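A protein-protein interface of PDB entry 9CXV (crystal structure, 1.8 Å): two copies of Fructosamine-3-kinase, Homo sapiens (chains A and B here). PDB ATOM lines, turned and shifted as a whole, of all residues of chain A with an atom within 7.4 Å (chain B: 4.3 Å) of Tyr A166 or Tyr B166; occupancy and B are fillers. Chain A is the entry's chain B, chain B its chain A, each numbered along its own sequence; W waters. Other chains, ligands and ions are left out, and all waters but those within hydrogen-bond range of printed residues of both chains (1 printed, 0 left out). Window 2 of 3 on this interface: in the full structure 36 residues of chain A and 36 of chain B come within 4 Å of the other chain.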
ATOM      1  N   GLN A 158      -7.185   3.279 -31.377  1.00  0.00           N
ATOM      2  CA  GLN A 158      -7.113   4.719 -31.169  1.00  0.00           C
ATOM      3  C   GLN A 158      -8.388   5.410 -31.637  1.00  0.00           C
ATOM      4  O   GLN A 158      -8.867   6.357 -30.994  1.00  0.00           O
ATOM      5  CB  GLN A 158      -5.899   5.289 -31.924  1.00  0.00           C
ATOM      6  CG  GLN A 158      -4.542   4.736 -31.326  1.00  0.00           C
ATOM      7  CD  GLN A 158      -4.162   5.541 -30.066  1.00  0.00           C
ATOM      8  OE1 GLN A 158      -4.681   6.660 -29.853  1.00  0.00           O
ATOM      9  NE2 GLN A 158      -3.228   5.007 -29.261  1.00  0.00           N
ATOM     10  N   ASP A 160     -11.404   4.190 -31.917  1.00  0.00           N
ATOM     11  CA  ASP A 160     -12.543   3.937 -31.031  1.00  0.00           C
ATOM     12  C   ASP A 160     -12.526   4.874 -29.823  1.00  0.00           C
ATOM     13  O   ASP A 160     -13.597   5.320 -29.341  1.00  0.00           O
ATOM     14  CB  ASP A 160     -12.521   2.493 -30.552  1.00  0.00           C
ATOM     15  CG  ASP A 160     -13.024   1.506 -31.621  1.00  0.00           C
ATOM     16  OD1 ASP A 160     -13.573   1.924 -32.668  1.00  0.00           O
ATOM     17  OD2 ASP A 160     -12.810   0.302 -31.413  1.00  0.00           O
ATOM     18  N   LEU A 161     -11.334   5.130 -29.277  1.00  0.00           N
ATOM     19  CA  LEU A 161     -11.216   6.114 -28.190  1.00  0.00           C
ATOM     20  C   LEU A 161     -11.531   7.527 -28.665  1.00  0.00           C
ATOM     21  O   LEU A 161     -12.208   8.288 -27.959  1.00  0.00           O
ATOM     22  CB  LEU A 161      -9.801   5.986 -27.595  1.00  0.00           C
ATOM     23  CG  LEU A 161      -9.484   6.802 -26.380  1.00  0.00           C
ATOM     24  CD1 LEU A 161     -10.569   6.551 -25.315  1.00  0.00           C
ATOM     25  CD2 LEU A 161      -8.061   6.338 -25.910  1.00  0.00           C
ATOM     26  N   ILE A 162     -11.095   7.913 -29.868  1.00  0.00           N
ATOM     27  CA  ILE A 162     -11.532   9.203 -30.422  1.00  0.00           C
ATOM     28  C   ILE A 162     -13.051   9.272 -30.562  1.00  0.00           C
ATOM     29  O   ILE A 162     -13.667  10.322 -30.284  1.00  0.00           O
ATOM     30  CB  ILE A 162     -10.834   9.447 -31.773  1.00  0.00           C
ATOM     31  CG1 ILE A 162      -9.387   9.898 -31.467  1.00  0.00           C
ATOM     32  CG2 ILE A 162     -11.515  10.570 -32.611  1.00  0.00           C
ATOM     33  CD1 ILE A 162      -8.465   9.519 -32.527  1.00  0.00           C
ATOM     34  N   GLU A 163     -13.679   8.189 -31.011  1.00  0.00           N
ATOM     35  CA  GLU A 163     -15.152   8.215 -31.097  1.00  0.00           C
ATOM     36  C   GLU A 163     -15.754   8.356 -29.710  1.00  0.00           C
ATOM     37  O   GLU A 163     -16.675   9.157 -29.498  1.00  0.00           O
ATOM     38  CB  GLU A 163     -15.653   6.948 -31.793  1.00  0.00           C
ATOM     39  CG  GLU A 163     -17.214   6.805 -31.854  1.00  0.00           C
ATOM     40  CD  GLU A 163     -17.895   7.954 -32.574  1.00  0.00           C
ATOM     41  OE1 GLU A 163     -17.335   8.606 -33.487  1.00  0.00           O
ATOM     42  OE2 GLU A 163     -19.048   8.218 -32.230  1.00  0.00           O
ATOM     43  N   LYS A 164     -15.232   7.628 -28.742  1.00  0.00           N
ATOM     44  CA  LYS A 164     -15.813   7.725 -27.411  1.00  0.00           C
ATOM     45  C   LYS A 164     -15.636   9.130 -26.815  1.00  0.00           C
ATOM     46  O   LYS A 164     -16.575   9.694 -26.226  1.00  0.00           O
ATOM     47  CB  LYS A 164     -15.224   6.637 -26.516  1.00  0.00           C
ATOM     48  CG  LYS A 164     -15.451   6.928 -25.027  1.00  0.00           C
ATOM     49  CD  LYS A 164     -15.177   5.676 -24.160  1.00  0.00           C
ATOM     50  CE  LYS A 164     -13.707   5.482 -23.866  1.00  0.00           C
ATOM     51  NZ  LYS A 164     -13.201   6.294 -22.712  1.00  0.00           N
ATOM     52  N   ASP A 165     -14.474   9.745 -26.989  1.00  0.00           N
ATOM     53  CA  ASP A 165     -14.198  11.008 -26.296  1.00  0.00           C
ATOM     54  C   ASP A 165     -14.530  12.262 -27.099  1.00  0.00           C
ATOM     55  O   ASP A 165     -14.936  13.285 -26.507  1.00  0.00           O
ATOM     56  CB  ASP A 165     -12.712  11.033 -25.858  1.00  0.00           C
ATOM     57  CG  ASP A 165     -12.429  10.031 -24.739  1.00  0.00           C
ATOM     58  OD1 ASP A 165     -13.405   9.486 -24.167  1.00  0.00           O
ATOM     59  OD2 ASP A 165     -11.248   9.770 -24.408  1.00  0.00           O
ATOM     60  N   TYR A 166     -14.390  12.250 -28.421  1.00  0.00           N
ATOM     61  CA  TYR A 166     -14.628  13.419 -29.235  1.00  0.00           C
ATOM     62  C   TYR A 166     -15.816  13.271 -30.178  1.00  0.00           C
ATOM     63  O   TYR A 166     -16.197  14.260 -30.822  1.00  0.00           O
ATOM     64  CB  TYR A 166     -13.385  13.763 -30.067  1.00  0.00           C
ATOM     65  CG  TYR A 166     -12.118  14.022 -29.258  1.00  0.00           C
ATOM     66  CD1 TYR A 166     -11.252  12.976 -28.941  1.00  0.00           C
ATOM     67  CD2 TYR A 166     -11.816  15.313 -28.736  1.00  0.00           C
ATOM     68  CE1 TYR A 166     -10.063  13.193 -28.196  1.00  0.00           C
ATOM     69  CE2 TYR A 166     -10.622  15.535 -27.965  1.00  0.00           C
ATOM     70  CZ  TYR A 166      -9.765  14.473 -27.696  1.00  0.00           C
ATOM     71  OH  TYR A 166      -8.604  14.634 -26.960  1.00  0.00           O
ATOM     72  N   ALA A 167     -16.337  12.055 -30.346  1.00  0.00           N
ATOM     73  CA  ALA A 167     -17.445  11.746 -31.277  1.00  0.00           C
ATOM     74  C   ALA A 167     -17.271  12.433 -32.628  1.00  0.00           C
ATOM     75  O   ALA A 167     -18.185  13.082 -33.157  1.00  0.00           O
ATOM     76  CB  ALA A 167     -18.789  12.124 -30.632  1.00  0.00           C
ATOM     77  N   ASP A 168     -16.076  12.281 -33.212  1.00  0.00           N
ATOM     78  CA  ASP A 168     -15.671  13.078 -34.367  1.00  0.00           C
ATOM     79  C   ASP A 168     -16.148  12.439 -35.662  1.00  0.00           C
ATOM     80  O   ASP A 168     -15.624  11.396 -36.078  1.00  0.00           O
ATOM     81  CB  ASP A 168     -14.164  13.266 -34.382  1.00  0.00           C
ATOM     82  CG  ASP A 168     -13.752  14.351 -35.321  1.00  0.00           C
ATOM     83  OD1 ASP A 168     -13.727  14.067 -36.538  1.00  0.00           O
ATOM     84  OD2 ASP A 168     -13.431  15.480 -34.890  1.00  0.00           O
ATOM     85  N   ARG A 169     -17.155  13.050 -36.309  1.00  0.00           N
ATOM     86  CA  ARG A 169     -17.719  12.439 -37.515  1.00  0.00           C
ATOM     87  C   ARG A 169     -16.668  12.258 -38.602  1.00  0.00           C
ATOM     88  O   ARG A 169     -16.610  11.199 -39.255  1.00  0.00           O
ATOM     89  CB  ARG A 169     -18.882  13.291 -38.091  1.00  0.00           C
ATOM     90  CG  ARG A 169     -19.338  12.741 -39.486  1.00  0.00           C
ATOM     91  CD  ARG A 169     -20.560  13.519 -40.091  1.00  0.00           C
ATOM     92  NE  ARG A 169     -21.575  13.782 -39.073  1.00  0.00           N
ATOM     93  CZ  ARG A 169     -22.582  12.966 -38.770  1.00  0.00           C
ATOM     94  NH1 ARG A 169     -22.827  11.864 -39.471  1.00  0.00           N
ATOM     95  NH2 ARG A 169     -23.355  13.253 -37.720  1.00  0.00           N
ATOM     96  N   ARG A 172     -14.369   9.276 -38.097  1.00  0.00           N
ATOM     97  CA  ARG A 172     -15.114   8.045 -38.376  1.00  0.00           C
ATOM     98  C   ARG A 172     -15.203   7.776 -39.873  1.00  0.00           C
ATOM     99  O   ARG A 172     -14.962   6.643 -40.327  1.00  0.00           O
ATOM    100  CB  ARG A 172     -16.562   8.104 -37.832  1.00  0.00           C
ATOM    101  CG  ARG A 172     -16.825   7.654 -36.449  1.00  0.00           C
ATOM    102  CD  ARG A 172     -18.364   7.356 -36.268  1.00  0.00           C
ATOM    103  NE  ARG A 172     -19.198   8.369 -36.891  1.00  0.00           N
ATOM    104  CZ  ARG A 172     -19.594   9.491 -36.294  1.00  0.00           C
ATOM    105  NH1 ARG A 172     -19.184   9.811 -35.072  1.00  0.00           N
ATOM    106  NH2 ARG A 172     -20.410  10.323 -36.943  1.00  0.00           N
ATOM    107  N   LEU A 268      -2.902  10.076 -33.982  1.00  0.00           N
ATOM    108  CA  LEU A 268      -4.096   9.668 -33.245  1.00  0.00           C
ATOM    109  C   LEU A 268      -3.783   9.520 -31.767  1.00  0.00           C
ATOM    110  O   LEU A 268      -4.555   9.963 -30.891  1.00  0.00           O
ATOM    111  CB  LEU A 268      -4.657   8.353 -33.821  1.00  0.00           C
ATOM    112  CG  LEU A 268      -5.156   8.516 -35.287  1.00  0.00           C
ATOM    113  CD1 LEU A 268      -5.457   7.063 -35.798  1.00  0.00           C
ATOM    114  CD2 LEU A 268      -6.436   9.381 -35.418  1.00  0.00           C
ATOM    115  N   HIS A 270      -1.489  11.062 -30.158  1.00  0.00           N
ATOM    116  CA  HIS A 270      -1.291  12.390 -29.566  1.00  0.00           C
ATOM    117  C   HIS A 270      -2.610  13.126 -29.424  1.00  0.00           C
ATOM    118  O   HIS A 270      -2.806  13.881 -28.466  1.00  0.00           O
ATOM    119  CB  HIS A 270      -0.281  13.188 -30.423  1.00  0.00           C
ATOM    120  CG  HIS A 270       1.165  12.850 -30.113  1.00  0.00           C
ATOM    121  ND1 HIS A 270       1.696  11.569 -30.247  1.00  0.00           N
ATOM    122  CD2 HIS A 270       2.158  13.615 -29.591  1.00  0.00           C
ATOM    123  CE1 HIS A 270       2.953  11.572 -29.834  1.00  0.00           C
ATOM    124  NE2 HIS A 270       3.258  12.802 -29.430  1.00  0.00           N
ATOM    125  N   TRP A 271      -3.551  12.897 -30.331  1.00  0.00           N
ATOM    126  CA  TRP A 271      -4.894  13.444 -30.142  1.00  0.00           C
ATOM    127  C   TRP A 271      -5.511  12.894 -28.866  1.00  0.00           C
ATOM    128  O   TRP A 271      -6.099  13.647 -28.059  1.00  0.00           O
ATOM    129  CB  TRP A 271      -5.748  13.104 -31.368  1.00  0.00           C
ATOM    130  CG  TRP A 271      -7.160  13.756 -31.499  1.00  0.00           C
ATOM    131  CD1 TRP A 271      -7.837  14.562 -30.571  1.00  0.00           C
ATOM    132  CD2 TRP A 271      -8.032  13.613 -32.619  1.00  0.00           C
ATOM    133  NE1 TRP A 271      -9.093  14.914 -31.087  1.00  0.00           N
ATOM    134  CE2 TRP A 271      -9.233  14.341 -32.336  1.00  0.00           C
ATOM    135  CE3 TRP A 271      -7.926  12.935 -33.853  1.00  0.00           C
ATOM    136  CZ2 TRP A 271     -10.308  14.381 -33.242  1.00  0.00           C
ATOM    137  CZ3 TRP A 271      -8.997  12.988 -34.733  1.00  0.00           C
ATOM    138  CH2 TRP A 271     -10.167  13.709 -34.451  1.00  0.00           C
ATOM    139  N   ASN A 272      -5.408  11.587 -28.659  1.00  0.00           N
ATOM    140  CA  ASN A 272      -5.959  10.999 -27.459  1.00  0.00           C
ATOM    141  C   ASN A 272      -5.225  11.458 -26.195  1.00  0.00           C
ATOM    142  O   ASN A 272      -5.866  11.697 -25.169  1.00  0.00           O
ATOM    143  CB  ASN A 272      -5.967   9.488 -27.552  1.00  0.00           C
ATOM    144  CG  ASN A 272      -7.209   8.999 -28.320  1.00  0.00           C
ATOM    145  OD1 ASN A 272      -8.356   9.524 -28.087  1.00  0.00           O
ATOM    146  ND2 ASN A 272      -7.021   8.018 -29.227  1.00  0.00           N
ATOM    147  N   HIS A 273      -3.894  11.565 -26.236  1.00  0.00           N
ATOM    148  CA  HIS A 273      -3.171  11.971 -25.011  1.00  0.00           C
ATOM    149  C   HIS A 273      -3.265  13.470 -24.744  1.00  0.00           C
ATOM    150  O   HIS A 273      -3.387  13.898 -23.585  1.00  0.00           O
ATOM    151  CB  HIS A 273      -1.712  11.560 -25.126  1.00  0.00           C
ATOM    152  CG  HIS A 273      -1.465  10.157 -24.689  1.00  0.00           C
ATOM    153  ND1 HIS A 273      -1.544   9.090 -25.562  1.00  0.00           N
ATOM    154  CD2 HIS A 273      -1.183   9.628 -23.469  1.00  0.00           C
ATOM    155  CE1 HIS A 273      -1.292   7.969 -24.905  1.00  0.00           C
ATOM    156  NE2 HIS A 273      -1.052   8.269 -23.637  1.00  0.00           N
ATOM    157  N   PHE A 274      -3.190  14.287 -25.778  1.00  0.00           N
ATOM    158  CA  PHE A 274      -2.904  15.699 -25.647  1.00  0.00           C
ATOM    159  C   PHE A 274      -3.965  16.602 -26.229  1.00  0.00           C
ATOM    160  O   PHE A 274      -3.816  17.813 -26.097  1.00  0.00           O
ATOM    161  CB  PHE A 274      -1.546  16.061 -26.293  1.00  0.00           C
ATOM    162  CG  PHE A 274      -0.410  15.257 -25.770  1.00  0.00           C
ATOM    163  CD1 PHE A 274      -0.107  15.239 -24.406  1.00  0.00           C
ATOM    164  CD2 PHE A 274       0.363  14.490 -26.621  1.00  0.00           C
ATOM    165  CE1 PHE A 274       0.954  14.488 -23.900  1.00  0.00           C
ATOM    166  CE2 PHE A 274       1.443  13.699 -26.108  1.00  0.00           C
ATOM    167  CZ  PHE A 274       1.733  13.705 -24.750  1.00  0.00           C
ATOM    168  N   GLY A 275      -5.003  16.063 -26.905  1.00  0.00           N
ATOM    169  CA  GLY A 275      -6.199  16.842 -27.265  1.00  0.00           C
ATOM    170  C   GLY A 275      -6.270  17.329 -28.700  1.00  0.00           C
ATOM    171  O   GLY A 275      -5.461  16.965 -29.563  1.00  0.00           O
ATOM    172  N   ARG A 276      -7.253  18.219 -28.943  1.00  0.00           N
ATOM    173  CA  ARG A 276      -7.729  18.585 -30.284  1.00  0.00           C
ATOM    174  C   ARG A 276      -6.679  19.267 -31.169  1.00  0.00           C
ATOM    175  O   ARG A 276      -6.884  19.361 -32.395  1.00  0.00           O
ATOM    176  CB  ARG A 276      -8.958  19.535 -30.180  1.00  0.00           C
ATOM    177  N   GLU A 277      -5.614  19.789 -30.585  1.00  0.00           N
ATOM    178  CA  GLU A 277      -4.491  20.274 -31.356  1.00  0.00           C
ATOM    179  C   GLU A 277      -4.041  19.218 -32.379  1.00  0.00           C
ATOM    180  O   GLU A 277      -3.486  19.554 -33.426  1.00  0.00           O
ATOM    181  CB  GLU A 277      -3.333  20.555 -30.403  1.00  0.00           C
ATOM    182  CG  GLU A 277      -2.098  21.098 -31.032  1.00  0.00           C
ATOM    183  CD  GLU A 277      -0.921  21.101 -30.067  1.00  0.00           C
ATOM    184  OE1 GLU A 277      -1.122  20.747 -28.879  1.00  0.00           O
ATOM    185  OE2 GLU A 277       0.210  21.422 -30.505  1.00  0.00           O
ATOM    186  N   ARG A 279      -6.047  17.016 -33.893  1.00  0.00           N
ATOM    187  CA  ARG A 279      -7.097  16.639 -34.841  1.00  0.00           C
ATOM    188  C   ARG A 279      -6.692  16.948 -36.287  1.00  0.00           C
ATOM    189  O   ARG A 279      -6.840  16.100 -37.182  1.00  0.00           O
ATOM    190  CB  ARG A 279      -8.408  17.348 -34.452  1.00  0.00           C
ATOM    191  CG  ARG A 279      -9.493  17.207 -35.508  1.00  0.00           C
ATOM    192  CD  ARG A 279     -10.860  17.841 -35.019  1.00  0.00           C
ATOM    193  NE  ARG A 279     -11.973  17.388 -35.866  1.00  0.00           N
ATOM    194  CZ  ARG A 279     -12.295  17.959 -37.014  1.00  0.00           C
ATOM    195  NH1 ARG A 279     -11.584  18.966 -37.500  1.00  0.00           N
ATOM    196  NH2 ARG A 279     -13.341  17.499 -37.696  1.00  0.00           N
ATOM    197  N   ILE B 162     -19.152  23.587 -28.145  1.00  0.00           N
ATOM    198  CA  ILE B 162     -19.649  22.289 -27.693  1.00  0.00           C
ATOM    199  C   ILE B 162     -20.901  21.901 -28.465  1.00  0.00           C
ATOM    200  O   ILE B 162     -21.080  20.729 -28.837  1.00  0.00           O
ATOM    201  CB  ILE B 162     -19.912  22.271 -26.175  1.00  0.00           C
ATOM    202  CG1 ILE B 162     -18.585  22.073 -25.398  1.00  0.00           C
ATOM    203  CG2 ILE B 162     -20.801  21.092 -25.810  1.00  0.00           C
ATOM    204  CD1 ILE B 162     -18.667  22.676 -23.950  1.00  0.00           C
ATOM    205  N   GLU B 163     -21.772  22.870 -28.745  1.00  0.00           N
ATOM    206  CA  GLU B 163     -22.940  22.555 -29.554  1.00  0.00           C
ATOM    207  C   GLU B 163     -22.523  22.143 -30.973  1.00  0.00           C
ATOM    208  O   GLU B 163     -23.004  21.133 -31.504  1.00  0.00           O
ATOM    209  CB  GLU B 163     -23.898  23.748 -29.575  1.00  0.00           C
ATOM    210  CG  GLU B 163     -25.054  23.559 -30.551  1.00  0.00           C
ATOM    211  CD  GLU B 163     -26.095  22.519 -30.108  1.00  0.00           C
ATOM    212  OE1 GLU B 163     -25.980  21.902 -29.039  1.00  0.00           O
ATOM    213  OE2 GLU B 163     -27.043  22.269 -30.882  1.00  0.00           O
ATOM    214  N   LYS B 164     -21.637  22.924 -31.597  1.00  0.00           N
ATOM    215  CA  LYS B 164     -21.100  22.587 -32.914  1.00  0.00           C
ATOM    216  C   LYS B 164     -20.511  21.186 -32.958  1.00  0.00           C
ATOM    217  O   LYS B 164     -20.835  20.398 -33.854  1.00  0.00           O
ATOM    218  CB  LYS B 164     -20.054  23.635 -33.306  1.00  0.00           C
ATOM    219  CG  LYS B 164     -19.639  23.702 -34.809  1.00  0.00           C
ATOM    220  CD  LYS B 164     -18.318  24.471 -34.953  1.00  0.00           C
ATOM    221  CE  LYS B 164     -17.324  23.831 -35.904  1.00  0.00           C
ATOM    222  NZ  LYS B 164     -17.308  24.563 -37.197  1.00  0.00           N
ATOM    223  N   ASP B 165     -19.643  20.841 -32.005  1.00  0.00           N
ATOM    224  CA  ASP B 165     -18.879  19.603 -32.145  1.00  0.00           C
ATOM    225  C   ASP B 165     -19.536  18.401 -31.510  1.00  0.00           C
ATOM    226  O   ASP B 165     -19.234  17.276 -31.895  1.00  0.00           O
ATOM    227  CB  ASP B 165     -17.486  19.731 -31.532  1.00  0.00           C
ATOM    228  CG  ASP B 165     -16.591  20.601 -32.347  1.00  0.00           C
ATOM    229  OD1 ASP B 165     -16.928  20.835 -33.534  1.00  0.00           O
ATOM    230  OD2 ASP B 165     -15.561  21.060 -31.814  1.00  0.00           O
ATOM    231  N   TYR B 166     -20.373  18.594 -30.510  1.00  0.00           N
ATOM    232  CA  TYR B 166     -20.945  17.489 -29.778  1.00  0.00           C
ATOM    233  C   TYR B 166     -22.450  17.506 -29.806  1.00  0.00           C
ATOM    234  O   TYR B 166     -23.041  16.478 -29.472  1.00  0.00           O
ATOM    235  CB  TYR B 166     -20.509  17.473 -28.299  1.00  0.00           C
ATOM    236  CG  TYR B 166     -19.034  17.305 -28.094  1.00  0.00           C
ATOM    237  CD1 TYR B 166     -18.198  18.400 -28.112  1.00  0.00           C
ATOM    238  CD2 TYR B 166     -18.476  16.040 -27.885  1.00  0.00           C
ATOM    239  CE1 TYR B 166     -16.845  18.277 -27.940  1.00  0.00           C
ATOM    240  CE2 TYR B 166     -17.094  15.889 -27.706  1.00  0.00           C
ATOM    241  CZ  TYR B 166     -16.294  17.007 -27.759  1.00  0.00           C
ATOM    242  OH  TYR B 166     -14.954  16.896 -27.577  1.00  0.00           O
ATOM    243  N   ALA B 167     -23.082  18.644 -30.143  1.00  0.00           N
ATOM    244  CA  ALA B 167     -24.550  18.784 -30.140  1.00  0.00           C
ATOM    245  C   ALA B 167     -25.151  18.244 -28.842  1.00  0.00           C
ATOM    246  O   ALA B 167     -26.090  17.444 -28.837  1.00  0.00           O
ATOM    247  CB  ALA B 167     -25.165  18.092 -31.366  1.00  0.00           C
ATOM    248  N   ASP B 168     -24.590  18.688 -27.715  1.00  0.00           N
ATOM    249  CA  ASP B 168     -24.961  18.147 -26.415  1.00  0.00           C
ATOM    250  C   ASP B 168     -26.235  18.836 -25.919  1.00  0.00           C
ATOM    251  O   ASP B 168     -26.251  20.064 -25.715  1.00  0.00           O
ATOM    252  CB  ASP B 168     -23.795  18.296 -25.435  1.00  0.00           C
ATOM    253  CG  ASP B 168     -23.984  17.480 -24.192  1.00  0.00           C
ATOM    254  OD1 ASP B 168     -24.825  17.898 -23.366  1.00  0.00           O
ATOM    255  OD2 ASP B 168     -23.303  16.443 -23.998  1.00  0.00           O
ATOM    256  N   TRP B 271     -13.275  20.333 -21.821  1.00  0.00           N
ATOM    257  CA  TRP B 271     -14.122  19.539 -22.702  1.00  0.00           C
ATOM    258  C   TRP B 271     -13.776  19.813 -24.161  1.00  0.00           C
ATOM    259  O   TRP B 271     -13.572  18.876 -24.944  1.00  0.00           O
ATOM    260  CB  TRP B 271     -15.599  19.825 -22.412  1.00  0.00           C
ATOM    261  CG  TRP B 271     -16.648  18.983 -23.108  1.00  0.00           C
ATOM    262  CD1 TRP B 271     -16.467  18.063 -24.137  1.00  0.00           C
ATOM    263  CD2 TRP B 271     -18.052  19.012 -22.834  1.00  0.00           C
ATOM    264  NE1 TRP B 271     -17.689  17.511 -24.496  1.00  0.00           N
ATOM    265  CE2 TRP B 271     -18.677  18.087 -23.717  1.00  0.00           C
ATOM    266  CE3 TRP B 271     -18.866  19.768 -21.937  1.00  0.00           C
ATOM    267  CZ2 TRP B 271     -20.067  17.891 -23.721  1.00  0.00           C
ATOM    268  CZ3 TRP B 271     -20.232  19.558 -21.933  1.00  0.00           C
ATOM    269  CH2 TRP B 271     -20.834  18.626 -22.830  1.00  0.00           C
ATOM    270  N   HIS B 273     -11.011  20.934 -25.379  1.00  0.00           N
ATOM    271  CA  HIS B 273      -9.631  20.541 -25.721  1.00  0.00           C
ATOM    272  C   HIS B 273      -9.435  19.027 -25.698  1.00  0.00           C
ATOM    273  O   HIS B 273      -8.688  18.475 -26.526  1.00  0.00           O
ATOM    274  CB  HIS B 273      -8.621  21.176 -24.754  1.00  0.00           C
ATOM    275  CG  HIS B 273      -8.176  22.544 -25.155  1.00  0.00           C
ATOM    276  ND1 HIS B 273      -8.915  23.684 -24.863  1.00  0.00           N
ATOM    277  CD2 HIS B 273      -7.087  22.967 -25.845  1.00  0.00           C
ATOM    278  CE1 HIS B 273      -8.275  24.745 -25.332  1.00  0.00           C
ATOM    279  NE2 HIS B 273      -7.174  24.335 -25.946  1.00  0.00           N
ATOM    280  N   PHE B 274     -10.022  18.355 -24.718  1.00  0.00           N
ATOM    281  CA  PHE B 274      -9.659  16.989 -24.354  1.00  0.00           C
ATOM    282  C   PHE B 274     -10.843  16.037 -24.427  1.00  0.00           C
ATOM    283  O   PHE B 274     -10.679  14.838 -24.177  1.00  0.00           O
ATOM    284  CB  PHE B 274      -9.034  16.972 -22.946  1.00  0.00           C
ATOM    285  CG  PHE B 274      -7.905  17.938 -22.792  1.00  0.00           C
ATOM    286  CD1 PHE B 274      -6.778  17.839 -23.618  1.00  0.00           C
ATOM    287  CD2 PHE B 274      -7.945  18.947 -21.848  1.00  0.00           C
ATOM    288  CE1 PHE B 274      -5.729  18.754 -23.531  1.00  0.00           C
ATOM    289  CE2 PHE B 274      -6.895  19.841 -21.724  1.00  0.00           C
ATOM    290  CZ  PHE B 274      -5.776  19.752 -22.571  1.00  0.00           C
ATOM    291  N   GLY B 275     -12.035  16.542 -24.732  1.00  0.00           N
ATOM    292  CA  GLY B 275     -13.195  15.699 -24.951  1.00  0.00           C
ATOM    293  C   GLY B 275     -14.016  15.389 -23.711  1.00  0.00           C
ATOM    294  O   GLY B 275     -13.961  16.060 -22.676  1.00  0.00           O
ATOM    295  N   ARG B 276     -14.799  14.326 -23.835  1.00  0.00           N
ATOM    296  CA  ARG B 276     -15.950  14.090 -22.965  1.00  0.00           C
ATOM    297  C   ARG B 276     -15.593  13.617 -21.557  1.00  0.00           C
ATOM    298  O   ARG B 276     -16.503  13.553 -20.712  1.00  0.00           O
ATOM    299  CB  ARG B 276     -16.901  13.097 -23.661  1.00  0.00           C
ATOM    300  CG  ARG B 276     -17.925  13.756 -24.614  1.00  0.00           C
ATOM    301  CD  ARG B 276     -18.751  12.714 -25.434  1.00  0.00           C
HETATM  302  O   HOH W   1      -8.335  13.375 -24.781  1.00  0.00           O
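N of Arg B276 sits at hydrogen-bond distance from O of Asp A165 (2.9 Å). The backbone carbonyl oxygen of His B273 is in hydrogen-bond range of the backbone NH of Arg A276 (2.8 Å). The backbone carbonyl oxygen (O) of Phe B274 is in hydrogen-bond range of the side-chain hydroxyl (OH) of Tyr A166.
O of His A270 is in hydrogen-bond range of N of Gly A275, 3.5 Å away. NZ of Lys A164 is in salt-bridge range of OD1 of Asp A165, 3.5 Å away. The side-chain hydroxyl (OH) of Tyr A166 sits at hydrogen-bond distance from the backbone carbonyl oxygen (O) of Trp A271, at 2.9 Å.
Among the printed residues, pairs that only touch across the chains: Gly A275 with His B273 (3.1 Å), Phe A274 with Phe B274 (3.3 Å), Asp A165 with Gly B275 (3.4 Å), Asp A165 with Tyr B166 (3.6 Å), Tyr A166 with Tyr B166 (3.6 Å), Tyr A166 with Gly B275 (3.7 Å), Tyr A166 with His B273 (3.8 Å), Lys A164 with Arg B276 (3.8 Å) and Gly A275 with Phe B274 (3.8 Å).
Of the printed residues of chain B, Lys A164 touches Arg B276 (3.8 Å). Of chain B, only Tyr B166 (3.6 Å), His B273 (3.8 Å), Phe B274 (3.5 Å) and Gly B275 (3.7 Å) come within 4 Å of Tyr A166. Printed residues of chain B within 4 Å of Phe A274: Phe B274 (3.3 Å). Of the printed residues of chain B, Gly A275 touches His B273 and Phe B274. Glu A277 touches none of the printed residues of chain B. Tyr B166 touches just these residues of chain A: Asp A165 and Tyr A166. No residue of chain A comes within 4 Å of Ala B167. Of the printed residues of chain A, His B273 touches Tyr A166 (3.8 Å), Gly A275 (3.1 Å) and Arg A276 (2.8 Å). Of the printed residues of chain A, Phe B274 touches Tyr A166 (3.5 Å), Phe A274 (3.3 Å) and Gly A275 (3.8 Å). The nearest printed residue of chain B that does not touch Tyr A166 is Asp B165 (4.4 Å). The nearest residue of chain A that does not touch Tyr B166 is Ala A167 (4.7 Å). The nearest printed residue of chain A that does not touch His B273 is Phe A274 (4.9 Å).
Of the 22 printed residues of chain A, 6 touch a printed residue of chain B. Hydrophobic or aromatic side chains of chain A within 4 Å of the printed part of chain B: Tyr A166. Of the 12 printed residues of chain B, 5 touch a printed residue of chain A. Among the printed residues, no Asp or Glu carboxylate lies within 4 Å of a Lys or Arg side-chain nitrogen of the other chain.
Tyr B166 touches its own counterpart, Tyr A166. Tyr A166 touches Phe B274, but with the chains exchanged Phe A274 does not touch Tyr B166 (11.1 Å). Tyr A166 touches Gly B275, but with the chains exchanged Gly A275 does not touch Tyr B166 (8.8 Å). Gly A275 touches Phe B274, but with the chains exchanged Phe A274 does not touch Gly B275 (8.2 Å). Positions printed for both chains: 162, 163, 164, 165, 166, 167, 168, 271, 273, 274, 275 and 276. Of the 12 pairs that touch across the chains among the printed residues, 2 have their exchanged pair printed and touching as well.
Water W1 lies within hydrogen-bond range of the side-chain hydroxyl (OH) of Tyr A166 (2.5 Å), the backbone carbonyl oxygen (O) of Phe B274 (2.8 Å) and the backbone carbonyl oxygen (O) of Asn A272 (3.0 Å).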
